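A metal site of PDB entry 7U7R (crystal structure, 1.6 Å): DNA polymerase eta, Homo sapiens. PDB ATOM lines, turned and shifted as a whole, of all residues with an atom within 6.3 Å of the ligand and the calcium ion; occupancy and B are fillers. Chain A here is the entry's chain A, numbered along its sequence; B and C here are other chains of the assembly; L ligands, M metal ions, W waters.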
ATOM      1  N   ASP A  16     -27.623  11.251   5.292  1.00  0.00           N
ATOM      2  CA  ASP A  16     -27.132  11.805   4.026  1.00  0.00           C
ATOM      3  C   ASP A  16     -26.194  10.791   3.370  1.00  0.00           C
ATOM      4  O   ASP A  16     -25.181  10.414   3.954  1.00  0.00           O
ATOM      5  CB  ASP A  16     -26.416  13.130   4.299  1.00  0.00           C
ATOM      6  CG  ASP A  16     -26.056  13.877   3.044  1.00  0.00           C
ATOM      7  OD1 ASP A  16     -26.442  13.421   1.952  1.00  0.00           O
ATOM      8  OD2 ASP A  16     -25.445  14.967   3.175  1.00  0.00           O
ATOM      9  N   MET A  17     -26.506  10.402   2.130  1.00  0.00           N
ATOM     10  CA  MET A  17     -25.629   9.413   1.505  1.00  0.00           C
ATOM     11  C   MET A  17     -24.277  10.047   1.185  1.00  0.00           C
ATOM     12  O   MET A  17     -24.226  11.195   0.755  1.00  0.00           O
ATOM     13  CB  MET A  17     -26.296   8.852   0.229  1.00  0.00           C
ATOM     14  CG  MET A  17     -27.732   8.440   0.443  1.00  0.00           C
ATOM     15  SD  MET A  17     -27.841   7.059   1.614  1.00  0.00           S
ATOM     16  CE  MET A  17     -26.755   5.908   0.852  1.00  0.00           C
ATOM     17  N   ASP A  18     -23.197   9.340   1.440  1.00  0.00           N
ATOM     18  CA  ASP A  18     -21.861   9.893   1.096  1.00  0.00           C
ATOM     19  C   ASP A  18     -21.685   9.916  -0.428  1.00  0.00           C
ATOM     20  O   ASP A  18     -22.029   8.902  -1.033  1.00  0.00           O
ATOM     21  CB  ASP A  18     -20.752   9.071   1.736  1.00  0.00           C
ATOM     22  CG  ASP A  18     -20.850   8.978   3.252  1.00  0.00           C
ATOM     23  OD1 ASP A  18     -21.298   9.953   3.861  1.00  0.00           O
ATOM     24  OD2 ASP A  18     -20.465   7.935   3.795  1.00  0.00           O
ATOM     25  N   CYS A  19     -21.103  10.986  -0.968  1.00  0.00           N
ATOM     26  CA  CYS A  19     -20.799  11.108  -2.422  1.00  0.00           C
ATOM     27  C   CYS A  19     -21.781  10.246  -3.227  1.00  0.00           C
ATOM     28  O   CYS A  19     -21.318   9.392  -3.970  1.00  0.00           O
ATOM     29  CB  CYS A  19     -19.322  10.821  -2.689  1.00  0.00           C
ATOM     30  SG  CYS A  19     -18.659   9.279  -2.024  1.00  0.00           S
ATOM     31  N   PHE A  20     -23.079  10.539  -3.145  1.00  0.00           N
ATOM     32  CA  PHE A  20     -24.126   9.631  -3.691  1.00  0.00           C
ATOM     33  C   PHE A  20     -23.922   9.193  -5.148  1.00  0.00           C
ATOM     34  O   PHE A  20     -23.789   7.996  -5.368  1.00  0.00           O
ATOM     35  CB  PHE A  20     -25.531  10.212  -3.510  1.00  0.00           C
ATOM     36  CG  PHE A  20     -26.631   9.223  -3.802  1.00  0.00           C
ATOM     37  CD1 PHE A  20     -26.587   7.939  -3.279  1.00  0.00           C
ATOM     38  CD2 PHE A  20     -27.705   9.558  -4.609  1.00  0.00           C
ATOM     39  CE1 PHE A  20     -27.583   7.018  -3.550  1.00  0.00           C
ATOM     40  CE2 PHE A  20     -28.710   8.633  -4.880  1.00  0.00           C
ATOM     41  CZ  PHE A  20     -28.649   7.363  -4.350  1.00  0.00           C
ATOM     42  N   PHE A  21     -23.932  10.133  -6.084  1.00  0.00           N
ATOM     43  CA  PHE A  21     -23.840   9.716  -7.509  1.00  0.00           C
ATOM     44  C   PHE A  21     -22.569   8.877  -7.717  1.00  0.00           C
ATOM     45  O   PHE A  21     -22.608   7.936  -8.493  1.00  0.00           O
ATOM     46  CB  PHE A  21     -23.915  10.934  -8.439  1.00  0.00           C
ATOM     47  CG  PHE A  21     -25.269  11.591  -8.596  1.00  0.00           C
ATOM     48  CD1 PHE A  21     -26.246  11.466  -7.632  1.00  0.00           C
ATOM     49  CD2 PHE A  21     -25.548  12.365  -9.706  1.00  0.00           C
ATOM     50  CE1 PHE A  21     -27.470  12.088  -7.771  1.00  0.00           C
ATOM     51  CE2 PHE A  21     -26.782  12.983  -9.859  1.00  0.00           C
ATOM     52  CZ  PHE A  21     -27.741  12.841  -8.888  1.00  0.00           C
ATOM     53  N   VAL A  22     -21.480   9.234  -7.038  1.00  0.00           N
ATOM     54  CA  VAL A  22     -20.221   8.446  -7.141  1.00  0.00           C
ATOM     55  C   VAL A  22     -20.473   7.004  -6.649  1.00  0.00           C
ATOM     56  O   VAL A  22     -20.098   6.076  -7.343  1.00  0.00           O
ATOM     57  CB  VAL A  22     -19.064   9.107  -6.370  1.00  0.00           C
ATOM     58  CG1 VAL A  22     -17.924   8.136  -6.122  1.00  0.00           C
ATOM     59  CG2 VAL A  22     -18.562  10.347  -7.077  1.00  0.00           C
ATOM     60  N   GLN A  41     -21.343  15.897 -15.614  1.00  0.00           N
ATOM     61  CA  GLN A  41     -22.358  15.969 -16.661  1.00  0.00           C
ATOM     62  C   GLN A  41     -21.806  16.687 -17.887  1.00  0.00           C
ATOM     63  O   GLN A  41     -21.163  17.743 -17.770  1.00  0.00           O
ATOM     64  CB  GLN A  41     -23.700  16.543 -16.149  1.00  0.00           C
ATOM     65  CG  GLN A  41     -23.715  17.716 -15.260  1.00  0.00           C
ATOM     66  CD  GLN A  41     -25.057  17.876 -14.491  1.00  0.00           C
ATOM     67  OE1 GLN A  41     -25.957  16.997 -14.470  1.00  0.00           O
ATOM     68  NE2 GLN A  41     -25.195  19.021 -13.900  1.00  0.00           N
ATOM     69  N   ILE A  51     -20.155  17.070 -10.488  1.00  0.00           N
ATOM     70  CA  ILE A  51     -21.227  17.249  -9.511  1.00  0.00           C
ATOM     71  C   ILE A  51     -21.119  16.343  -8.290  1.00  0.00           C
ATOM     72  O   ILE A  51     -21.890  16.538  -7.339  1.00  0.00           O
ATOM     73  CB  ILE A  51     -22.621  17.100 -10.158  1.00  0.00           C
ATOM     74  CG1 ILE A  51     -22.756  15.773 -10.908  1.00  0.00           C
ATOM     75  CG2 ILE A  51     -22.956  18.309 -11.057  1.00  0.00           C
ATOM     76  CD1 ILE A  51     -24.162  15.474 -11.379  1.00  0.00           C
ATOM     77  N   ALA A  52     -20.180  15.401  -8.247  1.00  0.00           N
ATOM     78  CA  ALA A  52     -20.005  14.540  -7.080  1.00  0.00           C
ATOM     79  C   ALA A  52     -18.582  14.022  -7.087  1.00  0.00           C
ATOM     80  O   ALA A  52     -18.023  13.779  -8.169  1.00  0.00           O
ATOM     81  CB  ALA A  52     -21.007  13.376  -7.065  1.00  0.00           C
ATOM     82  N   VAL A  53     -17.988  13.842  -5.900  1.00  0.00           N
ATOM     83  CA  VAL A  53     -16.546  13.598  -5.756  1.00  0.00           C
ATOM     84  C   VAL A  53     -16.312  12.592  -4.627  1.00  0.00           C
ATOM     85  O   VAL A  53     -16.720  12.837  -3.488  1.00  0.00           O
ATOM     86  CB  VAL A  53     -15.797  14.899  -5.419  1.00  0.00           C
ATOM     87  CG1 VAL A  53     -14.302  14.661  -5.426  1.00  0.00           C
ATOM     88  CG2 VAL A  53     -16.155  15.977  -6.411  1.00  0.00           C
ATOM     89  N   TYR A  55     -14.235  10.603  -1.692  1.00  0.00           N
ATOM     90  CA  TYR A  55     -13.400  11.224  -0.659  1.00  0.00           C
ATOM     91  C   TYR A  55     -11.909  11.097  -0.996  1.00  0.00           C
ATOM     92  O   TYR A  55     -11.116  12.022  -0.717  1.00  0.00           O
ATOM     93  CB  TYR A  55     -13.770  10.611   0.705  1.00  0.00           C
ATOM     94  CG  TYR A  55     -15.057  11.242   1.233  1.00  0.00           C
ATOM     95  CD1 TYR A  55     -16.290  10.868   0.716  1.00  0.00           C
ATOM     96  CD2 TYR A  55     -15.035  12.257   2.177  1.00  0.00           C
ATOM     97  CE1 TYR A  55     -17.477  11.473   1.157  1.00  0.00           C
ATOM     98  CE2 TYR A  55     -16.221  12.863   2.632  1.00  0.00           C
ATOM     99  CZ  TYR A  55     -17.429  12.475   2.107  1.00  0.00           C
ATOM    100  OH  TYR A  55     -18.612  13.066   2.534  1.00  0.00           O
ATOM    101  N   ARG A  58     -11.430  14.024  -3.163  1.00  0.00           N
ATOM    102  CA  ARG A  58     -11.482  15.256  -2.374  1.00  0.00           C
ATOM    103  C   ARG A  58     -10.131  15.555  -1.731  1.00  0.00           C
ATOM    104  O   ARG A  58      -9.768  16.722  -1.565  1.00  0.00           O
ATOM    105  CB  ARG A  58     -12.570  15.162  -1.301  1.00  0.00           C
ATOM    106  CG  ARG A  58     -13.971  15.050  -1.843  1.00  0.00           C
ATOM    107  CD  ARG A  58     -14.999  14.971  -0.737  1.00  0.00           C
ATOM    108  NE  ARG A  58     -16.306  14.623  -1.259  1.00  0.00           N
ATOM    109  CZ  ARG A  58     -17.452  14.783  -0.604  1.00  0.00           C
ATOM    110  NH1 ARG A  58     -17.464  15.275   0.624  1.00  0.00           N
ATOM    111  NH2 ARG A  58     -18.586  14.419  -1.189  1.00  0.00           N
ATOM    112  N   ARG A  64     -17.106  19.606  -6.262  1.00  0.00           N
ATOM    113  CA  ARG A  64     -18.282  19.936  -7.036  1.00  0.00           C
ATOM    114  C   ARG A  64     -18.115  21.290  -7.712  1.00  0.00           C
ATOM    115  O   ARG A  64     -17.424  22.178  -7.194  1.00  0.00           O
ATOM    116  CB  ARG A  64     -19.471  19.900  -6.081  1.00  0.00           C
ATOM    117  CG  ARG A  64     -20.776  20.295  -6.640  1.00  0.00           C
ATOM    118  CD  ARG A  64     -21.698  20.703  -5.515  1.00  0.00           C
ATOM    119  NE  ARG A  64     -22.895  21.270  -6.113  1.00  0.00           N
ATOM    120  CZ  ARG A  64     -23.094  22.569  -6.249  1.00  0.00           C
ATOM    121  NH1 ARG A  64     -22.274  23.458  -5.721  1.00  0.00           N
ATOM    122  NH2 ARG A  64     -24.147  22.982  -6.953  1.00  0.00           N
ATOM    123  N   SER A  65     -18.726  21.457  -8.892  1.00  0.00           N
ATOM    124  CA  SER A  65     -18.750  22.673  -9.689  1.00  0.00           C
ATOM    125  C   SER A  65     -17.435  22.893 -10.430  1.00  0.00           C
ATOM    126  O   SER A  65     -17.329  23.872 -11.153  1.00  0.00           O
ATOM    127  CB  SER A  65     -19.031  23.930  -8.850  1.00  0.00           C
ATOM    128  OG  SER A  65     -20.144  23.694  -8.003  1.00  0.00           O
ATOM    129  N   LEU A  92     -31.127  11.980 -15.136  1.00  0.00           N
ATOM    130  CA  LEU A  92     -30.709  11.539 -13.797  1.00  0.00           C
ATOM    131  C   LEU A  92     -31.530  10.363 -13.264  1.00  0.00           C
ATOM    132  O   LEU A  92     -31.567  10.141 -12.050  1.00  0.00           O
ATOM    133  CB  LEU A  92     -30.758  12.702 -12.821  1.00  0.00           C
ATOM    134  CG  LEU A  92     -30.042  13.979 -13.268  1.00  0.00           C
ATOM    135  CD1 LEU A  92     -30.288  15.125 -12.305  1.00  0.00           C
ATOM    136  CD2 LEU A  92     -28.564  13.731 -13.458  1.00  0.00           C
ATOM    137  N   SER A 116     -33.767  15.838  -0.022  1.00  0.00           N
ATOM    138  CA  SER A 116     -33.153  15.946  -1.339  1.00  0.00           C
ATOM    139  C   SER A 116     -32.995  14.541  -1.877  1.00  0.00           C
ATOM    140  O   SER A 116     -33.302  13.557  -1.182  1.00  0.00           O
ATOM    141  CB  SER A 116     -31.807  16.686  -1.273  1.00  0.00           C
ATOM    142  OG  SER A 116     -30.769  15.818  -0.855  1.00  0.00           O
ATOM    143  N   ILE A 117     -32.480  14.429  -3.104  1.00  0.00           N
ATOM    144  CA  ILE A 117     -32.273  13.113  -3.719  1.00  0.00           C
ATOM    145  C   ILE A 117     -31.541  12.135  -2.803  1.00  0.00           C
ATOM    146  O   ILE A 117     -31.745  10.920  -2.903  1.00  0.00           O
ATOM    147  CB  ILE A 117     -31.524  13.254  -5.057  1.00  0.00           C
ATOM    148  CG1 ILE A 117     -31.711  11.974  -5.870  1.00  0.00           C
ATOM    149  CG2 ILE A 117     -30.044  13.571  -4.860  1.00  0.00           C
ATOM    150  CD1 ILE A 117     -31.410  12.163  -7.335  1.00  0.00           C
ATOM    151  N   ASP A 118     -30.686  12.617  -1.914  1.00  0.00           N
ATOM    152  CA  ASP A 118     -29.978  11.597  -1.137  1.00  0.00           C
ATOM    153  C   ASP A 118     -29.959  11.919   0.344  1.00  0.00           C
ATOM    154  O   ASP A 118     -29.119  11.395   1.097  1.00  0.00           O
ATOM    155  CB  ASP A 118     -28.562  11.387  -1.645  1.00  0.00           C
ATOM    156  CG  ASP A 118     -27.646  12.472  -1.200  1.00  0.00           C
ATOM    157  OD1 ASP A 118     -28.092  13.638  -1.073  1.00  0.00           O
ATOM    158  OD2 ASP A 118     -26.469  12.152  -0.943  1.00  0.00           O
ATOM    159  N   GLU A 119     -30.930  12.698   0.805  1.00  0.00           N
ATOM    160  CA  GLU A 119     -30.925  12.902   2.241  1.00  0.00           C
ATOM    161  C   GLU A 119     -32.342  13.022   2.739  1.00  0.00           C
ATOM    162  O   GLU A 119     -33.236  13.528   2.046  1.00  0.00           O
ATOM    163  CB  GLU A 119     -30.102  14.126   2.649  1.00  0.00           C
ATOM    164  CG  GLU A 119     -30.835  15.410   2.556  1.00  0.00           C
ATOM    165  CD  GLU A 119     -29.944  16.614   2.728  1.00  0.00           C
ATOM    166  OE1 GLU A 119     -28.995  16.787   1.955  1.00  0.00           O
ATOM    167  OE2 GLU A 119     -30.175  17.382   3.670  1.00  0.00           O
ATOM    168  N   SER A 216     -23.689   9.001   6.090  1.00  0.00           N
ATOM    169  CA  SER A 216     -23.418   9.632   7.364  1.00  0.00           C
ATOM    170  C   SER A 216     -24.755  10.052   7.960  1.00  0.00           C
ATOM    171  O   SER A 216     -25.759  10.115   7.261  1.00  0.00           O
ATOM    172  CB  SER A 216     -22.494  10.838   7.181  1.00  0.00           C
ATOM    173  OG  SER A 216     -21.244  10.433   6.645  1.00  0.00           O
ATOM    174  N   LYS A 227     -28.707  18.125  10.984  1.00  0.00           N
ATOM    175  CA  LYS A 227     -27.983  18.349   9.728  1.00  0.00           C
ATOM    176  C   LYS A 227     -26.544  18.767  10.016  1.00  0.00           C
ATOM    177  O   LYS A 227     -25.580  18.230   9.425  1.00  0.00           O
ATOM    178  CB  LYS A 227     -28.711  19.421   8.921  1.00  0.00           C
ATOM    179  CG  LYS A 227     -28.035  19.867   7.616  1.00  0.00           C
ATOM    180  CD  LYS A 227     -27.924  18.711   6.652  1.00  0.00           C
ATOM    181  CE  LYS A 227     -27.407  19.174   5.282  1.00  0.00           C
ATOM    182  NZ  LYS A 227     -27.248  18.035   4.329  1.00  0.00           N
ATOM    183  N   LYS A 234     -17.989  13.070   8.451  1.00  0.00           N
ATOM    184  CA  LYS A 234     -18.145  12.331   7.219  1.00  0.00           C
ATOM    185  C   LYS A 234     -16.791  11.792   6.762  1.00  0.00           C
ATOM    186  O   LYS A 234     -15.758  12.396   7.030  1.00  0.00           O
ATOM    187  CB  LYS A 234     -18.721  13.262   6.150  1.00  0.00           C
ATOM    188  CG  LYS A 234     -20.258  13.341   6.115  1.00  0.00           C
ATOM    189  CD  LYS A 234     -20.791  13.899   4.783  1.00  0.00           C
ATOM    190  CE  LYS A 234     -22.272  13.520   4.559  1.00  0.00           C
ATOM    191  NZ  LYS A 234     -22.527  12.428   3.522  1.00  0.00           N
ATOM    192  N   PRO A 235     -16.767  10.649   6.034  1.00  0.00           N
ATOM    193  CA  PRO A 235     -17.869   9.791   5.595  1.00  0.00           C
ATOM    194  C   PRO A 235     -18.111   8.596   6.494  1.00  0.00           C
ATOM    195  O   PRO A 235     -17.269   8.262   7.345  1.00  0.00           O
ATOM    196  CB  PRO A 235     -17.391   9.309   4.221  1.00  0.00           C
ATOM    197  CG  PRO A 235     -15.896   9.108   4.453  1.00  0.00           C
ATOM    198  CD  PRO A 235     -15.493  10.220   5.413  1.00  0.00           C
ATOM    199  P    DT B   8     -25.813  22.923   0.807  1.00  0.00           P
ATOM    200  OP1  DT B   8     -25.392  22.635   2.225  1.00  0.00           O
ATOM    201  OP2  DT B   8     -24.859  23.871   0.066  1.00  0.00           O
ATOM    202  O5'  DT B   8     -25.732  21.492   0.053  1.00  0.00           O
ATOM    203  C5'  DT B   8     -26.843  21.026  -0.756  1.00  0.00           C
ATOM    204  C4'  DT B   8     -26.302  20.553  -2.090  1.00  0.00           C
ATOM    205  O4'  DT B   8     -26.948  21.295  -3.149  1.00  0.00           O
ATOM    206  C3'  DT B   8     -24.801  20.755  -2.278  1.00  0.00           C
ATOM    207  O3'  DT B   8     -24.169  19.693  -2.990  1.00  0.00           O
ATOM    208  C2'  DT B   8     -24.740  21.985  -3.165  1.00  0.00           C
ATOM    209  C1'  DT B   8     -25.940  21.733  -4.042  1.00  0.00           C
ATOM    210  N1   DT B   8     -26.404  22.908  -4.786  1.00  0.00           N
ATOM    211  C2   DT B   8     -27.260  22.706  -5.841  1.00  0.00           C
ATOM    212  O2   DT B   8     -27.705  21.604  -6.127  1.00  0.00           O
ATOM    213  N3   DT B   8     -27.592  23.847  -6.525  1.00  0.00           N
ATOM    214  C4   DT B   8     -27.146  25.121  -6.281  1.00  0.00           C
ATOM    215  O4   DT B   8     -27.542  26.051  -6.975  1.00  0.00           O
ATOM    216  C5   DT B   8     -26.231  25.255  -5.169  1.00  0.00           C
ATOM    217  C7   DT B   8     -25.704  26.613  -4.825  1.00  0.00           C
ATOM    218  C6   DT B   8     -25.902  24.150  -4.493  1.00  0.00           C
ATOM    219  P    DT C   4     -23.152  26.014 -16.227  1.00  0.00           P
ATOM    220  OP1  DT C   4     -22.298  26.180 -17.415  1.00  0.00           O
ATOM    221  OP2  DT C   4     -23.935  27.147 -15.674  1.00  0.00           O
ATOM    222  O5'  DT C   4     -24.137  24.809 -16.572  1.00  0.00           O
ATOM    223  C5'  DT C   4     -23.612  23.475 -16.724  1.00  0.00           C
ATOM    224  C4'  DT C   4     -24.650  22.435 -16.380  1.00  0.00           C
ATOM    225  O4'  DT C   4     -24.656  22.185 -14.953  1.00  0.00           O
ATOM    226  C3'  DT C   4     -26.096  22.778 -16.740  1.00  0.00           C
ATOM    227  O3'  DT C   4     -26.662  21.546 -17.179  1.00  0.00           O
ATOM    228  C2'  DT C   4     -26.682  23.257 -15.426  1.00  0.00           C
ATOM    229  C1'  DT C   4     -25.958  22.406 -14.422  1.00  0.00           C
ATOM    230  N1   DT C   4     -25.787  23.025 -13.108  1.00  0.00           N
ATOM    231  C2   DT C   4     -25.761  22.215 -12.007  1.00  0.00           C
ATOM    232  O2   DT C   4     -25.923  21.008 -12.059  1.00  0.00           O
ATOM    233  N3   DT C   4     -25.558  22.872 -10.823  1.00  0.00           N
ATOM    234  C4   DT C   4     -25.366  24.227 -10.637  1.00  0.00           C
ATOM    235  O4   DT C   4     -25.199  24.675  -9.514  1.00  0.00           O
ATOM    236  C5   DT C   4     -25.392  25.020 -11.850  1.00  0.00           C
ATOM    237  C7   DT C   4     -25.208  26.505 -11.753  1.00  0.00           C
ATOM    238  C6   DT C   4     -25.589  24.380 -13.006  1.00  0.00           C
ATOM    239  P    DA C   5     -28.231  21.429 -17.707  1.00  0.00           P
ATOM    240  OP1  DA C   5     -28.250  20.633 -18.942  1.00  0.00           O
ATOM    241  OP2  DA C   5     -28.888  22.757 -17.691  1.00  0.00           O
ATOM    242  O5'  DA C   5     -28.946  20.591 -16.555  1.00  0.00           O
ATOM    243  C5'  DA C   5     -28.437  19.334 -16.093  1.00  0.00           C
ATOM    244  C4'  DA C   5     -29.285  18.809 -14.962  1.00  0.00           C
ATOM    245  O4'  DA C   5     -28.969  19.544 -13.750  1.00  0.00           O
ATOM    246  C3'  DA C   5     -30.800  18.951 -15.170  1.00  0.00           C
ATOM    247  O3'  DA C   5     -31.433  17.741 -14.722  1.00  0.00           O
ATOM    248  C2'  DA C   5     -31.154  20.175 -14.334  1.00  0.00           C
ATOM    249  C1'  DA C   5     -30.150  20.116 -13.202  1.00  0.00           C
ATOM    250  N9   DA C   5     -29.793  21.419 -12.652  1.00  0.00           N
ATOM    251  C8   DA C   5     -29.730  22.618 -13.304  1.00  0.00           C
ATOM    252  N7   DA C   5     -29.375  23.625 -12.543  1.00  0.00           N
ATOM    253  C5   DA C   5     -29.199  23.044 -11.295  1.00  0.00           C
ATOM    254  C6   DA C   5     -28.816  23.564 -10.049  1.00  0.00           C
ATOM    255  N6   DA C   5     -28.540  24.859  -9.849  1.00  0.00           N
ATOM    256  N1   DA C   5     -28.718  22.718  -9.007  1.00  0.00           N
ATOM    257  C2   DA C   5     -28.994  21.422  -9.206  1.00  0.00           C
ATOM    258  N3   DA C   5     -29.368  20.804 -10.336  1.00  0.00           N
ATOM    259  C4   DA C   5     -29.444  21.681 -11.345  1.00  0.00           C
ATOM    260  P    DT C   6     -33.044  17.546 -14.764  1.00  0.00           P
ATOM    261  OP1  DT C   6     -33.341  16.210 -14.232  1.00  0.00           O
ATOM    262  OP2  DT C   6     -33.549  17.934 -16.091  1.00  0.00           O
ATOM    263  O5'  DT C   6     -33.586  18.662 -13.788  1.00  0.00           O
ATOM    264  C5'  DT C   6     -34.565  18.394 -12.811  1.00  0.00           C
ATOM    265  C4'  DT C   6     -34.016  18.586 -11.417  1.00  0.00           C
ATOM    266  O4'  DT C   6     -33.152  19.735 -11.312  1.00  0.00           O
ATOM    267  C3'  DT C   6     -35.137  18.816 -10.418  1.00  0.00           C
ATOM    268  O3'  DT C   6     -35.270  17.579  -9.734  1.00  0.00           O
ATOM    269  C2'  DT C   6     -34.611  19.903  -9.498  1.00  0.00           C
ATOM    270  C1'  DT C   6     -33.200  20.164  -9.975  1.00  0.00           C
ATOM    271  N1   DT C   6     -32.842  21.597  -9.946  1.00  0.00           N
ATOM    272  C2   DT C   6     -32.366  22.110  -8.767  1.00  0.00           C
ATOM    273  O2   DT C   6     -32.213  21.440  -7.755  1.00  0.00           O
ATOM    274  N3   DT C   6     -32.051  23.444  -8.797  1.00  0.00           N
ATOM    275  C4   DT C   6     -32.165  24.298  -9.882  1.00  0.00           C
ATOM    276  O4   DT C   6     -31.850  25.470  -9.778  1.00  0.00           O
ATOM    277  C5   DT C   6     -32.683  23.686 -11.091  1.00  0.00           C
ATOM    278  C7   DT C   6     -32.848  24.542 -12.308  1.00  0.00           C
ATOM    279  C6   DT C   6     -33.000  22.390 -11.055  1.00  0.00           C
HETATM  280  N1  LIG L   1     -26.449  19.438 -10.199  1.00  0.00           N
HETATM  281  C1  LIG L   1     -26.876  18.137 -10.265  1.00  0.00           C
HETATM  282  N2  LIG L   1     -27.516  17.793 -11.387  1.00  0.00           N
HETATM  283  N3  LIG L   1     -26.699  17.204  -9.328  1.00  0.00           N
HETATM  284  C2  LIG L   1     -26.076  17.647  -8.252  1.00  0.00           C
HETATM  285  C3  LIG L   1     -25.603  18.899  -8.051  1.00  0.00           C
HETATM  286  C4  LIG L   1     -25.808  19.835  -9.085  1.00  0.00           C
HETATM  287  O1  LIG L   1     -25.443  21.017  -8.991  1.00  0.00           O
HETATM  288  N4  LIG L   1     -25.009  18.998  -6.796  1.00  0.00           N
HETATM  289  C5  LIG L   1     -25.118  17.788  -6.291  1.00  0.00           C
HETATM  290  N5  LIG L   1     -25.750  16.920  -7.131  1.00  0.00           N
HETATM  291  P1  LIG L   1     -24.835  16.130  -1.980  1.00  0.00           P
HETATM  292  P2  LIG L   1     -22.680  14.150  -2.107  1.00  0.00           P
HETATM  293  P3  LIG L   1     -21.435  14.237   0.517  1.00  0.00           P
HETATM  294  C6  LIG L   1     -25.981  15.492  -6.966  1.00  0.00           C
HETATM  295  O2  LIG L   1     -25.326  15.478  -0.759  1.00  0.00           O
HETATM  296  O3  LIG L   1     -23.737  13.193  -1.751  1.00  0.00           O
HETATM  297  O4  LIG L   1     -20.756  13.011   0.971  1.00  0.00           O
HETATM  298  C7  LIG L   1     -24.694  14.682  -6.879  1.00  0.00           C
HETATM  299  O5  LIG L   1     -24.776  17.717  -1.748  1.00  0.00           O
HETATM  300  O6  LIG L   1     -21.960  13.770  -3.438  1.00  0.00           O
HETATM  301  O7  LIG L   1     -20.673  15.515   0.939  1.00  0.00           O
HETATM  302  C8  LIG L   1     -24.575  14.326  -5.410  1.00  0.00           C
HETATM  303  O8  LIG L   1     -23.988  13.036  -5.297  1.00  0.00           O
HETATM  304  N6  LIG L   1     -23.312  15.638  -2.346  1.00  0.00           N
HETATM  305  O9  LIG L   1     -21.491  14.304  -1.077  1.00  0.00           O
HETATM  306  O10 LIG L   1     -22.910  14.305   0.962  1.00  0.00           O
HETATM  307  C9  LIG L   1     -26.034  14.288  -4.954  1.00  0.00           C
HETATM  308  O11 LIG L   1     -26.688  15.304  -5.741  1.00  0.00           O
HETATM  309  C10 LIG L   1     -26.261  14.583  -3.491  1.00  0.00           C
HETATM  310  O12 LIG L   1     -25.801  15.915  -3.201  1.00  0.00           O
HETATM  311 CA    CA M   1     -24.845  13.304   0.285  1.00  0.00          CA
HETATM  312  O   HOH W   1     -28.224  17.373  -1.598  1.00  0.00           O
HETATM  313  O   HOH W   2     -20.012  17.618  -0.459  1.00  0.00           O
HETATM  314  O   HOH W   3     -22.072  17.124  -4.515  1.00  0.00           O
HETATM  315  O   HOH W   4     -28.461  17.249  -4.650  1.00  0.00           O
HETATM  316  O   HOH W   5     -19.610  14.773  -3.712  1.00  0.00           O
HETATM  317  O   HOH W   6     -23.554  16.556   1.954  1.00  0.00           O
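The backbone carbonyl oxygen (O) of Val 53 lies within hydrogen-bond range of the guanidinium group (NE) of Arg 58, at 2.9 Å.
O4 of DT 4 of chain C is in hydrogen-bond range of the guanidinium group (NH2) of Arg 64 (3.2 Å).
The side-chain carboxylate (OD1) of Asp 18 is in salt-bridge range of the side-chain amino group (NZ) of Lys 234 (2.8 Å).
The backbone NH (N) of Asp 118 sits close to the side-chain hydroxyl (OG) of Ser 116, at 3.4 Å.
O2 of DT 4 of chain C lies within hydrogen-bond range of NE2 of Gln 41 (2.8 Å).
The side-chain amino group (NZ) of Lys 227 is in salt-bridge range of the side-chain carboxylate (OD2) of Asp 16 (3.7 Å).
OD2 of Asp 16 is in salt-bridge range of NZ of Lys 234 (3.9 Å).
NH2 of Arg 64 sits at hydrogen-bond distance from N1 of DT 8 of chain B.
Of the 28 residues printed, 3 come within 4 Å of the calcium ion.
The nearest printed residue that does not touch the calcium ion is Lys 234 (4.1 Å).
O4' of DA 5 of chain C lies within hydrogen-bond range of a nitrogen (N2) of the ligand (3.3 Å).
An oxygen (O8) of the ligand lies within hydrogen-bond range of the backbone NH (N) of Phe 21 (3.0 Å).
The guanidinium group (NH2) of Arg 64 sits at hydrogen-bond distance from an oxygen (O1) of the ligand (3.1 Å).
O4 of the ligand lies within hydrogen-bond range of OH of Tyr 55, 2.7 Å away.
NH2 of Arg 58 is in salt-bridge range of O7 of the ligand (3.2 Å).
O3' of DT 8 of chain B lies close to O5 of the ligand.
An oxygen (O4) of the ligand sits at hydrogen-bond distance from the backbone NH (N) of Cys 19 (2.8 Å).
An oxygen (O4) of the ligand lies within salt-bridge range of the side-chain amino group (NZ) of Lys 234 (3.2 Å).
The backbone NH of Phe 20 lies within hydrogen-bond range of an oxygen (O8) of the ligand (3.4 Å).
N3 of DA 5 of chain C is in hydrogen-bond range of a nitrogen (N1) of the ligand.
O2 of DT 4 of chain C is in hydrogen-bond range of a nitrogen (N1) of the ligand (2.5 Å).
Water W6 lies within hydrogen-bond range of OD2 of Asp 16 (2.8 Å) and O7 of the ligand (3.2 Å).
Water W5 lies within hydrogen-bond range of O6 of the ligand, NH2 of Arg 58 and N of Val 53.
Water W3 lies within hydrogen-bond range of O of Ile 51 (2.9 Å) and N6 of the ligand (2.9 Å).
Water W1 lies within hydrogen-bond range of the side-chain hydroxyl of Ser 116 and an oxygen (O12) of the ligand.
The calcium ion is bound by O of Met 17 (2.2 Å), O10 of the ligand (2.3 Å), OD1 of Asp 16 (2.3 Å), O3 of the ligand (2.3 Å), OD2 of Asp 118 (2.3 Å) and O2 of the ligand (2.5 Å).
The calcium ion has six donor atoms within binding distance.
Merely in contact with the ligand: Asp 18, Ile 51, Ala 52, Gln 41, Ile 117 and Leu 92.
19 residues have an atom within 4 Å of the ligand: Asp 16, Met 17, Asp 18, Cys 19, Phe 20, Phe 21, Gln 41, Ile 51, Ala 52, Tyr 55, Arg 58, Arg 64, Leu 92, Ile 117, Asp 118, Lys 234, DT 8 of chain B, DT 4 of chain C and DA 5 of chain C.
Along chain A the residues within 4 Å of the ligand span positions 16 to 234.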
